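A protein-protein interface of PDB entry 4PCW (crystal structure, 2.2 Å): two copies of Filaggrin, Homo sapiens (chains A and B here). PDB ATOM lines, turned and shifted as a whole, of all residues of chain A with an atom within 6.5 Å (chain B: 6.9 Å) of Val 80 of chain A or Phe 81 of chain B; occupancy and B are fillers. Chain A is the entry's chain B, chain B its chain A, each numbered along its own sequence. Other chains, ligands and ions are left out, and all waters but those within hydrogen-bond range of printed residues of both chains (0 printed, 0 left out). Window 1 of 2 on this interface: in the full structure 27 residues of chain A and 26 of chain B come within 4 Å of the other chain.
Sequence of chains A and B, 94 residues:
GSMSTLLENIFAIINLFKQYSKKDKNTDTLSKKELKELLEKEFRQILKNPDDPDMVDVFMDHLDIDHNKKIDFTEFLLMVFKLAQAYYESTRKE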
ATOM      1  N   ILE A  10     -20.167  -4.429 -25.237  1.00  0.00           N
ATOM      2  CA  ILE A  10     -20.837  -5.722 -25.220  1.00  0.00           C
ATOM      3  C   ILE A  10     -19.799  -6.839 -25.279  1.00  0.00           C
ATOM      4  O   ILE A  10     -19.866  -7.801 -24.516  1.00  0.00           O
ATOM      5  CB  ILE A  10     -21.834  -5.850 -26.390  1.00  0.00           C
ATOM      6  CG1 ILE A  10     -23.048  -4.951 -26.138  1.00  0.00           C
ATOM      7  CG2 ILE A  10     -22.279  -7.301 -26.571  1.00  0.00           C
ATOM      8  CD1 ILE A  10     -23.973  -4.796 -27.327  1.00  0.00           C
ATOM      9  N   ILE A  13     -17.829  -7.260 -22.062  1.00  0.00           N
ATOM     10  CA  ILE A  13     -18.582  -8.032 -21.085  1.00  0.00           C
ATOM     11  C   ILE A  13     -18.512  -9.519 -21.419  1.00  0.00           C
ATOM     12  O   ILE A  13     -18.404 -10.356 -20.524  1.00  0.00           O
ATOM     13  CB  ILE A  13     -20.055  -7.571 -21.023  1.00  0.00           C
ATOM     14  CG1 ILE A  13     -20.131  -6.147 -20.469  1.00  0.00           C
ATOM     15  CG2 ILE A  13     -20.888  -8.507 -20.143  1.00  0.00           C
ATOM     16  CD1 ILE A  13     -21.485  -5.489 -20.635  1.00  0.00           C
ATOM     17  N   LEU A  16     -14.976 -10.758 -20.667  1.00  0.00           N
ATOM     18  CA  LEU A  16     -14.784 -10.776 -19.225  1.00  0.00           C
ATOM     19  C   LEU A  16     -15.301 -12.086 -18.646  1.00  0.00           C
ATOM     20  O   LEU A  16     -14.660 -12.696 -17.795  1.00  0.00           O
ATOM     21  CB  LEU A  16     -15.490  -9.586 -18.572  1.00  0.00           C
ATOM     22  CG  LEU A  16     -15.655  -9.629 -17.051  1.00  0.00           C
ATOM     23  CD1 LEU A  16     -15.473  -8.244 -16.464  1.00  0.00           C
ATOM     24  CD2 LEU A  16     -17.020 -10.178 -16.663  1.00  0.00           C
ATOM     25  N   PHE A  73     -23.823 -17.886 -19.016  1.00  0.00           N
ATOM     26  CA  PHE A  73     -23.738 -16.504 -19.469  1.00  0.00           C
ATOM     27  C   PHE A  73     -25.047 -15.752 -19.238  1.00  0.00           C
ATOM     28  O   PHE A  73     -25.037 -14.602 -18.801  1.00  0.00           O
ATOM     29  CB  PHE A  73     -23.357 -16.458 -20.950  1.00  0.00           C
ATOM     30  CG  PHE A  73     -22.934 -15.097 -21.428  1.00  0.00           C
ATOM     31  CD1 PHE A  73     -21.868 -14.439 -20.833  1.00  0.00           C
ATOM     32  CD2 PHE A  73     -23.586 -14.483 -22.484  1.00  0.00           C
ATOM     33  CE1 PHE A  73     -21.472 -13.192 -21.273  1.00  0.00           C
ATOM     34  CE2 PHE A  73     -23.192 -13.232 -22.930  1.00  0.00           C
ATOM     35  CZ  PHE A  73     -22.134 -12.587 -22.323  1.00  0.00           C
ATOM     36  N   GLU A  75     -27.342 -16.342 -17.002  1.00  0.00           N
ATOM     37  CA  GLU A  75     -27.437 -16.119 -15.563  1.00  0.00           C
ATOM     38  C   GLU A  75     -26.521 -14.976 -15.133  1.00  0.00           C
ATOM     39  O   GLU A  75     -26.863 -14.189 -14.251  1.00  0.00           O
ATOM     40  CB  GLU A  75     -27.081 -17.398 -14.796  1.00  0.00           C
ATOM     41  CG  GLU A  75     -28.177 -18.466 -14.807  1.00  0.00           C
ATOM     42  CD  GLU A  75     -27.728 -19.800 -14.221  1.00  0.00           C
ATOM     43  OE1 GLU A  75     -26.548 -20.171 -14.399  1.00  0.00           O
ATOM     44  OE2 GLU A  75     -28.559 -20.480 -13.581  1.00  0.00           O
ATOM     45  N   PHE A  76     -25.358 -14.892 -15.769  1.00  0.00           N
ATOM     46  CA  PHE A  76     -24.402 -13.828 -15.495  1.00  0.00           C
ATOM     47  C   PHE A  76     -24.957 -12.487 -15.961  1.00  0.00           C
ATOM     48  O   PHE A  76     -24.870 -11.489 -15.245  1.00  0.00           O
ATOM     49  CB  PHE A  76     -23.064 -14.140 -16.176  1.00  0.00           C
ATOM     50  CG  PHE A  76     -22.131 -12.967 -16.270  1.00  0.00           C
ATOM     51  CD1 PHE A  76     -21.344 -12.601 -15.193  1.00  0.00           C
ATOM     52  CD2 PHE A  76     -22.024 -12.248 -17.447  1.00  0.00           C
ATOM     53  CE1 PHE A  76     -20.475 -11.530 -15.285  1.00  0.00           C
ATOM     54  CE2 PHE A  76     -21.159 -11.176 -17.544  1.00  0.00           C
ATOM     55  CZ  PHE A  76     -20.383 -10.817 -16.462  1.00  0.00           C
ATOM     56  N   LEU A  77     -25.553 -12.472 -17.149  1.00  0.00           N
ATOM     57  CA  LEU A  77     -26.088 -11.239 -17.716  1.00  0.00           C
ATOM     58  C   LEU A  77     -27.205 -10.667 -16.850  1.00  0.00           C
ATOM     59  O   LEU A  77     -27.472  -9.465 -16.891  1.00  0.00           O
ATOM     60  CB  LEU A  77     -26.602 -11.473 -19.138  1.00  0.00           C
ATOM     61  CG  LEU A  77     -25.559 -11.674 -20.242  1.00  0.00           C
ATOM     62  CD1 LEU A  77     -26.254 -11.792 -21.586  1.00  0.00           C
ATOM     63  CD2 LEU A  77     -24.523 -10.549 -20.276  1.00  0.00           C
ATOM     64  N   LEU A  78     -27.846 -11.523 -16.060  1.00  0.00           N
ATOM     65  CA  LEU A  78     -28.887 -11.070 -15.148  1.00  0.00           C
ATOM     66  C   LEU A  78     -28.273 -10.133 -14.117  1.00  0.00           C
ATOM     67  O   LEU A  78     -28.850  -9.100 -13.776  1.00  0.00           O
ATOM     68  CB  LEU A  78     -29.556 -12.257 -14.453  1.00  0.00           C
ATOM     69  CG  LEU A  78     -31.032 -12.176 -14.034  1.00  0.00           C
ATOM     70  CD1 LEU A  78     -31.193 -12.674 -12.605  1.00  0.00           C
ATOM     71  CD2 LEU A  78     -31.641 -10.783 -14.180  1.00  0.00           C
ATOM     72  N   MET A  79     -27.091 -10.500 -13.635  1.00  0.00           N
ATOM     73  CA  MET A  79     -26.349  -9.663 -12.704  1.00  0.00           C
ATOM     74  C   MET A  79     -26.034  -8.321 -13.355  1.00  0.00           C
ATOM     75  O   MET A  79     -26.293  -7.263 -12.782  1.00  0.00           O
ATOM     76  CB  MET A  79     -25.059 -10.359 -12.269  1.00  0.00           C
ATOM     77  CG  MET A  79     -24.317  -9.657 -11.141  1.00  0.00           C
ATOM     78  SD  MET A  79     -22.558 -10.046 -11.103  1.00  0.00           S
ATOM     79  CE  MET A  79     -21.990  -9.174 -12.561  1.00  0.00           C
ATOM     80  N   VAL A  80     -25.489  -8.377 -14.565  1.00  0.00           N
ATOM     81  CA  VAL A  80     -25.075  -7.173 -15.274  1.00  0.00           C
ATOM     82  C   VAL A  80     -26.284  -6.282 -15.542  1.00  0.00           C
ATOM     83  O   VAL A  80     -26.194  -5.057 -15.457  1.00  0.00           O
ATOM     84  CB  VAL A  80     -24.374  -7.512 -16.603  1.00  0.00           C
ATOM     85  CG1 VAL A  80     -23.854  -6.246 -17.277  1.00  0.00           C
ATOM     86  CG2 VAL A  80     -23.232  -8.486 -16.366  1.00  0.00           C
ATOM     87  N   PHE A  81     -27.414  -6.908 -15.855  1.00  0.00           N
ATOM     88  CA  PHE A  81     -28.658  -6.186 -16.091  1.00  0.00           C
ATOM     89  C   PHE A  81     -29.082  -5.399 -14.856  1.00  0.00           C
ATOM     90  O   PHE A  81     -29.416  -4.220 -14.948  1.00  0.00           O
ATOM     91  CB  PHE A  81     -29.768  -7.158 -16.503  1.00  0.00           C
ATOM     92  CG  PHE A  81     -31.133  -6.529 -16.584  1.00  0.00           C
ATOM     93  CD1 PHE A  81     -31.515  -5.812 -17.707  1.00  0.00           C
ATOM     94  CD2 PHE A  81     -32.035  -6.663 -15.541  1.00  0.00           C
ATOM     95  CE1 PHE A  81     -32.772  -5.234 -17.783  1.00  0.00           C
ATOM     96  CE2 PHE A  81     -33.291  -6.091 -15.612  1.00  0.00           C
ATOM     97  CZ  PHE A  81     -33.660  -5.373 -16.733  1.00  0.00           C
ATOM     98  N   LYS A  82     -29.067  -6.060 -13.703  1.00  0.00           N
ATOM     99  CA  LYS A  82     -29.446  -5.425 -12.444  1.00  0.00           C
ATOM    100  C   LYS A  82     -28.543  -4.241 -12.101  1.00  0.00           C
ATOM    101  O   LYS A  82     -29.022  -3.199 -11.657  1.00  0.00           O
ATOM    102  CB  LYS A  82     -29.410  -6.447 -11.307  1.00  0.00           C
ATOM    103  CG  LYS A  82     -30.505  -7.489 -11.384  1.00  0.00           C
ATOM    104  CD  LYS A  82     -30.343  -8.540 -10.301  1.00  0.00           C
ATOM    105  CE  LYS A  82     -31.433  -9.592 -10.379  1.00  0.00           C
ATOM    106  NZ  LYS A  82     -32.789  -8.999 -10.215  1.00  0.00           N
ATOM    107  N   LEU A  83     -27.241  -4.405 -12.304  1.00  0.00           N
ATOM    108  CA  LEU A  83     -26.287  -3.344 -12.003  1.00  0.00           C
ATOM    109  C   LEU A  83     -26.530  -2.122 -12.873  1.00  0.00           C
ATOM    110  O   LEU A  83     -26.478  -0.989 -12.394  1.00  0.00           O
ATOM    111  CB  LEU A  83     -24.851  -3.833 -12.192  1.00  0.00           C
ATOM    112  CG  LEU A  83     -24.165  -4.471 -10.981  1.00  0.00           C
ATOM    113  CD1 LEU A  83     -22.827  -5.052 -11.376  1.00  0.00           C
ATOM    114  CD2 LEU A  83     -23.987  -3.463  -9.850  1.00  0.00           C
ATOM    115  N   ALA A  84     -26.791  -2.357 -14.155  1.00  0.00           N
ATOM    116  CA  ALA A  84     -27.046  -1.271 -15.090  1.00  0.00           C
ATOM    117  C   ALA A  84     -28.253  -0.450 -14.646  1.00  0.00           C
ATOM    118  O   ALA A  84     -28.214   0.780 -14.656  1.00  0.00           O
ATOM    119  CB  ALA A  84     -27.263  -1.818 -16.487  1.00  0.00           C
ATOM    120  N   GLN A  85     -29.319  -1.138 -14.249  1.00  0.00           N
ATOM    121  CA  GLN A  85     -30.532  -0.472 -13.791  1.00  0.00           C
ATOM    122  C   GLN A  85     -30.270   0.371 -12.551  1.00  0.00           C
ATOM    123  O   GLN A  85     -30.718   1.513 -12.459  1.00  0.00           O
ATOM    124  CB  GLN A  85     -31.626  -1.494 -13.485  1.00  0.00           C
ATOM    125  CG  GLN A  85     -32.281  -2.103 -14.704  1.00  0.00           C
ATOM    126  CD  GLN A  85     -33.514  -2.902 -14.342  1.00  0.00           C
ATOM    127  OE1 GLN A  85     -33.509  -3.666 -13.377  1.00  0.00           O
ATOM    128  NE2 GLN A  85     -34.586  -2.718 -15.103  1.00  0.00           N
ATOM    129  N   LEU B   6     -15.785  -4.340 -15.637  1.00  0.00           N
ATOM    130  CA  LEU B   6     -17.211  -4.527 -15.883  1.00  0.00           C
ATOM    131  C   LEU B   6     -17.994  -3.244 -15.612  1.00  0.00           C
ATOM    132  O   LEU B   6     -18.931  -2.914 -16.339  1.00  0.00           O
ATOM    133  CB  LEU B   6     -17.759  -5.663 -15.017  1.00  0.00           C
ATOM    134  CG  LEU B   6     -19.253  -5.968 -15.173  1.00  0.00           C
ATOM    135  CD1 LEU B   6     -19.570  -6.419 -16.590  1.00  0.00           C
ATOM    136  CD2 LEU B   6     -19.695  -7.020 -14.167  1.00  0.00           C
ATOM    137  N   ILE B  10     -20.491  -0.816 -18.029  1.00  0.00           N
ATOM    138  CA  ILE B  10     -21.865  -0.504 -17.649  1.00  0.00           C
ATOM    139  C   ILE B  10     -22.127   0.997 -17.671  1.00  0.00           C
ATOM    140  O   ILE B  10     -23.173   1.439 -18.139  1.00  0.00           O
ATOM    141  CB  ILE B  10     -22.200  -1.062 -16.250  1.00  0.00           C
ATOM    142  CG1 ILE B  10     -22.348  -2.584 -16.328  1.00  0.00           C
ATOM    143  CG2 ILE B  10     -23.489  -0.432 -15.698  1.00  0.00           C
ATOM    144  CD1 ILE B  10     -22.600  -3.263 -14.992  1.00  0.00           C
ATOM    145  N   ILE B  13     -22.388   2.121 -21.242  1.00  0.00           N
ATOM    146  CA  ILE B  13     -23.693   1.811 -21.811  1.00  0.00           C
ATOM    147  C   ILE B  13     -24.712   2.853 -21.356  1.00  0.00           C
ATOM    148  O   ILE B  13     -25.514   3.337 -22.154  1.00  0.00           O
ATOM    149  CB  ILE B  13     -24.157   0.394 -21.412  1.00  0.00           C
ATOM    150  CG1 ILE B  13     -23.279  -0.654 -22.096  1.00  0.00           C
ATOM    151  CG2 ILE B  13     -25.619   0.169 -21.804  1.00  0.00           C
ATOM    152  CD1 ILE B  13     -23.454  -2.070 -21.567  1.00  0.00           C
ATOM    153  N   THR B  74     -34.660   0.262 -19.528  1.00  0.00           N
ATOM    154  CA  THR B  74     -34.885  -1.169 -19.350  1.00  0.00           C
ATOM    155  C   THR B  74     -35.099  -1.857 -20.695  1.00  0.00           C
ATOM    156  O   THR B  74     -34.457  -2.865 -20.992  1.00  0.00           O
ATOM    157  CB  THR B  74     -36.096  -1.441 -18.440  1.00  0.00           C
ATOM    158  OG1 THR B  74     -35.888  -0.809 -17.173  1.00  0.00           O
ATOM    159  CG2 THR B  74     -36.289  -2.939 -18.228  1.00  0.00           C
ATOM    160  N   PHE B  76     -34.209  -0.767 -23.530  1.00  0.00           N
ATOM    161  CA  PHE B  76     -32.940  -0.654 -24.232  1.00  0.00           C
ATOM    162  C   PHE B  76     -31.997  -1.768 -23.792  1.00  0.00           C
ATOM    163  O   PHE B  76     -31.394  -2.446 -24.627  1.00  0.00           O
ATOM    164  CB  PHE B  76     -32.318   0.721 -23.980  1.00  0.00           C
ATOM    165  CG  PHE B  76     -30.919   0.860 -24.491  1.00  0.00           C
ATOM    166  CD1 PHE B  76     -30.675   1.017 -25.842  1.00  0.00           C
ATOM    167  CD2 PHE B  76     -29.845   0.851 -23.615  1.00  0.00           C
ATOM    168  CE1 PHE B  76     -29.386   1.152 -26.315  1.00  0.00           C
ATOM    169  CE2 PHE B  76     -28.555   0.986 -24.081  1.00  0.00           C
ATOM    170  CZ  PHE B  76     -28.323   1.136 -25.433  1.00  0.00           C
ATOM    171  N   LEU B  77     -31.888  -1.968 -22.482  1.00  0.00           N
ATOM    172  CA  LEU B  77     -31.013  -2.998 -21.930  1.00  0.00           C
ATOM    173  C   LEU B  77     -31.364  -4.398 -22.432  1.00  0.00           C
ATOM    174  O   LEU B  77     -30.471  -5.183 -22.754  1.00  0.00           O
ATOM    175  CB  LEU B  77     -31.064  -2.982 -20.401  1.00  0.00           C
ATOM    176  CG  LEU B  77     -30.312  -1.860 -19.678  1.00  0.00           C
ATOM    177  CD1 LEU B  77     -30.461  -2.025 -18.176  1.00  0.00           C
ATOM    178  CD2 LEU B  77     -28.841  -1.826 -20.061  1.00  0.00           C
ATOM    179  N   LEU B  78     -32.656  -4.714 -22.491  1.00  0.00           N
ATOM    180  CA  LEU B  78     -33.093  -6.029 -22.950  1.00  0.00           C
ATOM    181  C   LEU B  78     -32.507  -6.339 -24.324  1.00  0.00           C
ATOM    182  O   LEU B  78     -32.106  -7.471 -24.596  1.00  0.00           O
ATOM    183  CB  LEU B  78     -34.619  -6.111 -22.999  1.00  0.00           C
ATOM    184  CG  LEU B  78     -35.380  -6.065 -21.670  1.00  0.00           C
ATOM    185  CD1 LEU B  78     -36.876  -6.165 -21.931  1.00  0.00           C
ATOM    186  CD2 LEU B  78     -34.929  -7.165 -20.714  1.00  0.00           C
ATOM    187  N   MET B  79     -32.440  -5.324 -25.178  1.00  0.00           N
ATOM    188  CA  MET B  79     -31.876  -5.485 -26.513  1.00  0.00           C
ATOM    189  C   MET B  79     -30.359  -5.623 -26.443  1.00  0.00           C
ATOM    190  O   MET B  79     -29.773  -6.445 -27.147  1.00  0.00           O
ATOM    191  CB  MET B  79     -32.260  -4.304 -27.406  1.00  0.00           C
ATOM    192  CG  MET B  79     -31.855  -4.478 -28.863  1.00  0.00           C
ATOM    193  SD  MET B  79     -30.439  -3.473 -29.347  1.00  0.00           S
ATOM    194  CE  MET B  79     -31.170  -1.840 -29.383  1.00  0.00           C
ATOM    195  N   VAL B  80     -29.725  -4.821 -25.593  1.00  0.00           N
ATOM    196  CA  VAL B  80     -28.279  -4.880 -25.436  1.00  0.00           C
ATOM    197  C   VAL B  80     -27.837  -6.280 -25.019  1.00  0.00           C
ATOM    198  O   VAL B  80     -26.880  -6.826 -25.565  1.00  0.00           O
ATOM    199  CB  VAL B  80     -27.781  -3.860 -24.393  1.00  0.00           C
ATOM    200  CG1 VAL B  80     -26.300  -4.074 -24.088  1.00  0.00           C
ATOM    201  CG2 VAL B  80     -28.023  -2.438 -24.879  1.00  0.00           C
ATOM    202  N   PHE B  81     -28.538  -6.860 -24.054  1.00  0.00           N
ATOM    203  CA  PHE B  81     -28.135  -8.150 -23.514  1.00  0.00           C
ATOM    204  C   PHE B  81     -28.582  -9.305 -24.409  1.00  0.00           C
ATOM    205  O   PHE B  81     -28.077 -10.420 -24.281  1.00  0.00           O
ATOM    206  CB  PHE B  81     -28.676  -8.317 -22.094  1.00  0.00           C
ATOM    207  CG  PHE B  81     -28.070  -7.353 -21.112  1.00  0.00           C
ATOM    208  CD1 PHE B  81     -26.718  -7.410 -20.814  1.00  0.00           C
ATOM    209  CD2 PHE B  81     -28.844  -6.385 -20.498  1.00  0.00           C
ATOM    210  CE1 PHE B  81     -26.154  -6.523 -19.921  1.00  0.00           C
ATOM    211  CE2 PHE B  81     -28.283  -5.496 -19.604  1.00  0.00           C
ATOM    212  CZ  PHE B  81     -26.938  -5.566 -19.314  1.00  0.00           C
ATOM    213  N   LYS B  82     -29.511  -9.036 -25.322  1.00  0.00           N
ATOM    214  CA  LYS B  82     -29.856 -10.011 -26.354  1.00  0.00           C
ATOM    215  C   LYS B  82     -28.735 -10.112 -27.377  1.00  0.00           C
ATOM    216  O   LYS B  82     -28.403 -11.203 -27.841  1.00  0.00           O
ATOM    217  CB  LYS B  82     -31.155  -9.636 -27.061  1.00  0.00           C
ATOM    218  CG  LYS B  82     -32.389 -10.308 -26.504  1.00  0.00           C
ATOM    219  CD  LYS B  82     -33.371 -10.600 -27.617  1.00  0.00           C
ATOM    220  CE  LYS B  82     -34.783 -10.689 -27.099  1.00  0.00           C
ATOM    221  NZ  LYS B  82     -35.757 -10.828 -28.217  1.00  0.00           N
ATOM    222  N   LEU B  83     -28.163  -8.966 -27.738  1.00  0.00           N
ATOM    223  CA  LEU B  83     -27.027  -8.939 -28.649  1.00  0.00           C
ATOM    224  C   LEU B  83     -25.835  -9.626 -28.009  1.00  0.00           C
ATOM    225  O   LEU B  83     -25.171 -10.452 -28.637  1.00  0.00           O
ATOM    226  CB  LEU B  83     -26.668  -7.503 -29.028  1.00  0.00           C
ATOM    227  CG  LEU B  83     -27.500  -6.894 -30.157  1.00  0.00           C
ATOM    228  CD1 LEU B  83     -27.273  -5.396 -30.239  1.00  0.00           C
ATOM    229  CD2 LEU B  83     -27.166  -7.553 -31.486  1.00  0.00           C
ATOM    230  N   ALA B  84     -25.573  -9.279 -26.752  1.00  0.00           N
ATOM    231  CA  ALA B  84     -24.501  -9.899 -25.987  1.00  0.00           C
ATOM    232  C   ALA B  84     -24.685 -11.407 -25.991  1.00  0.00           C
ATOM    233  O   ALA B  84     -23.768 -12.162 -26.314  1.00  0.00           O
ATOM    234  CB  ALA B  84     -24.483  -9.365 -24.558  1.00  0.00           C
ATOM    235  N   GLN B  85     -25.896 -11.829 -25.650  1.00  0.00           N
ATOM    236  CA  GLN B  85     -26.240 -13.241 -25.590  1.00  0.00           C
ATOM    237  C   GLN B  85     -26.074 -13.896 -26.957  1.00  0.00           C
ATOM    238  O   GLN B  85     -25.699 -15.063 -27.054  1.00  0.00           O
ATOM    239  CB  GLN B  85     -27.675 -13.400 -25.082  1.00  0.00           C
ATOM    240  CG  GLN B  85     -28.125 -14.830 -24.861  1.00  0.00           C
ATOM    241  CD  GLN B  85     -29.482 -14.905 -24.183  1.00  0.00           C
ATOM    242  OE1 GLN B  85     -30.076 -13.880 -23.845  1.00  0.00           O
ATOM    243  NE2 GLN B  85     -29.977 -16.120 -23.980  1.00  0.00           N
ATOM    244  N   ALA B  86     -26.331 -13.124 -28.008  1.00  0.00           N
ATOM    245  CA  ALA B  86     -26.252 -13.623 -29.375  1.00  0.00           C
ATOM    246  C   ALA B  86     -24.813 -13.660 -29.879  1.00  0.00           C
ATOM    247  O   ALA B  86     -24.403 -14.624 -30.519  1.00  0.00           O
ATOM    248  CB  ALA B  86     -27.108 -12.770 -30.296  1.00  0.00           C
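Printed residues of chain A that touch a printed residue of chain B: Ile 10, Ile 13, Leu 16, Phe 73, Leu 77, Met 79, Val 80, Phe 81, Leu 83, Ala 84 and Gln 85. Hydrophobic or aromatic side chains of chain A that line the printed part of chain B: Ile 10, Ile 13, Leu 16, Phe 73, Leu 77, Met 79, Val 80, Phe 81, Leu 83 and Ala 84. Of the 15 printed residues of chain B, 7 touch a printed residue of chain A. Among the printed residues, 17 pairs touch across the chains. Among the printed residues, no Asp or Glu carboxylate lies within 4 Å of a Lys or Arg side-chain nitrogen of the other chain.
The side-chain amide nitrogen of Gln 85 of chain A is in hydrogen-bond range of the side-chain hydroxyl of Thr 74 of chain B (3.1 Å).
Ile 10 of chain A touches Ala 84 of chain B, and with the chains exchanged Ala 84 of chain A touches Ile 10 of chain B. Val 80 of chain A touches Phe 81 of chain B, but with the chains exchanged Phe 81 of chain A does not touch Val 80 of chain B (7.9 Å). Ala 84 of chain A touches Leu 77 of chain B, but with the chains exchanged Leu 77 of chain A does not touch Ala 84 of chain B (4.2 Å). Gln 85 of chain A touches Leu 77 of chain B, but with the chains exchanged Leu 77 of chain A does not touch Gln 85 of chain B (4.1 Å). Of the 17 pairs that touch across the chains among the printed residues, 7 have their exchanged pair printed and touching as well.
Leu 16 of chain A touches Leu 6 of chain B. Leu 77 of chain A touches Phe 81 of chain B. Met 79 of chain A touches Leu 6 of chain B (CE to CD2, 3.5 Å). Phe 81 of chain B touches Val 80 of chain A (CE1 to CG1, 3.5 Å). Phe 81 of chain A touches Thr 74 of chain B. CE1 of Phe 81 of chain A touches CB of Leu 77 of chain B (3.9 Å). Phe 81 of chain B touches Phe 81 of chain A. Leu 83 of chain A touches Ile 10 of chain B (CB to CD1, 3.6 Å). Ile 10 of chain B touches Ala 84 of chain A. Gln 85 of chain A touches Leu 77 of chain B.
Printed residues of chain B within 4 Å of Leu 16 of chain A: Leu 6 (3.7 Å). Printed residues of chain B within 4 Å of Phe 73 of chain A: Ala 84. Val 80 of chain A touches two residues of chain B. Of the printed residues of chain B, Ala 84 of chain A touches Ile 10 (3.7 Å) and Leu 77 (3.6 Å). Of the printed residues of chain A, Thr 74 of chain B touches Phe 81 (3.9 Å) and Gln 85 (3.1 Å). Of the printed residues of chain A, Phe 81 of chain B touches Leu 77, Val 80 and Phe 81. Lys 82 of chain B touches none of the printed residues of chain A. Of the printed residues of chain A, Ala 84 of chain B touches Ile 10 and Phe 73. The nearest residue of chain B that does not touch Val 80 of chain A is Leu 6 of chain B (4.2 Å).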
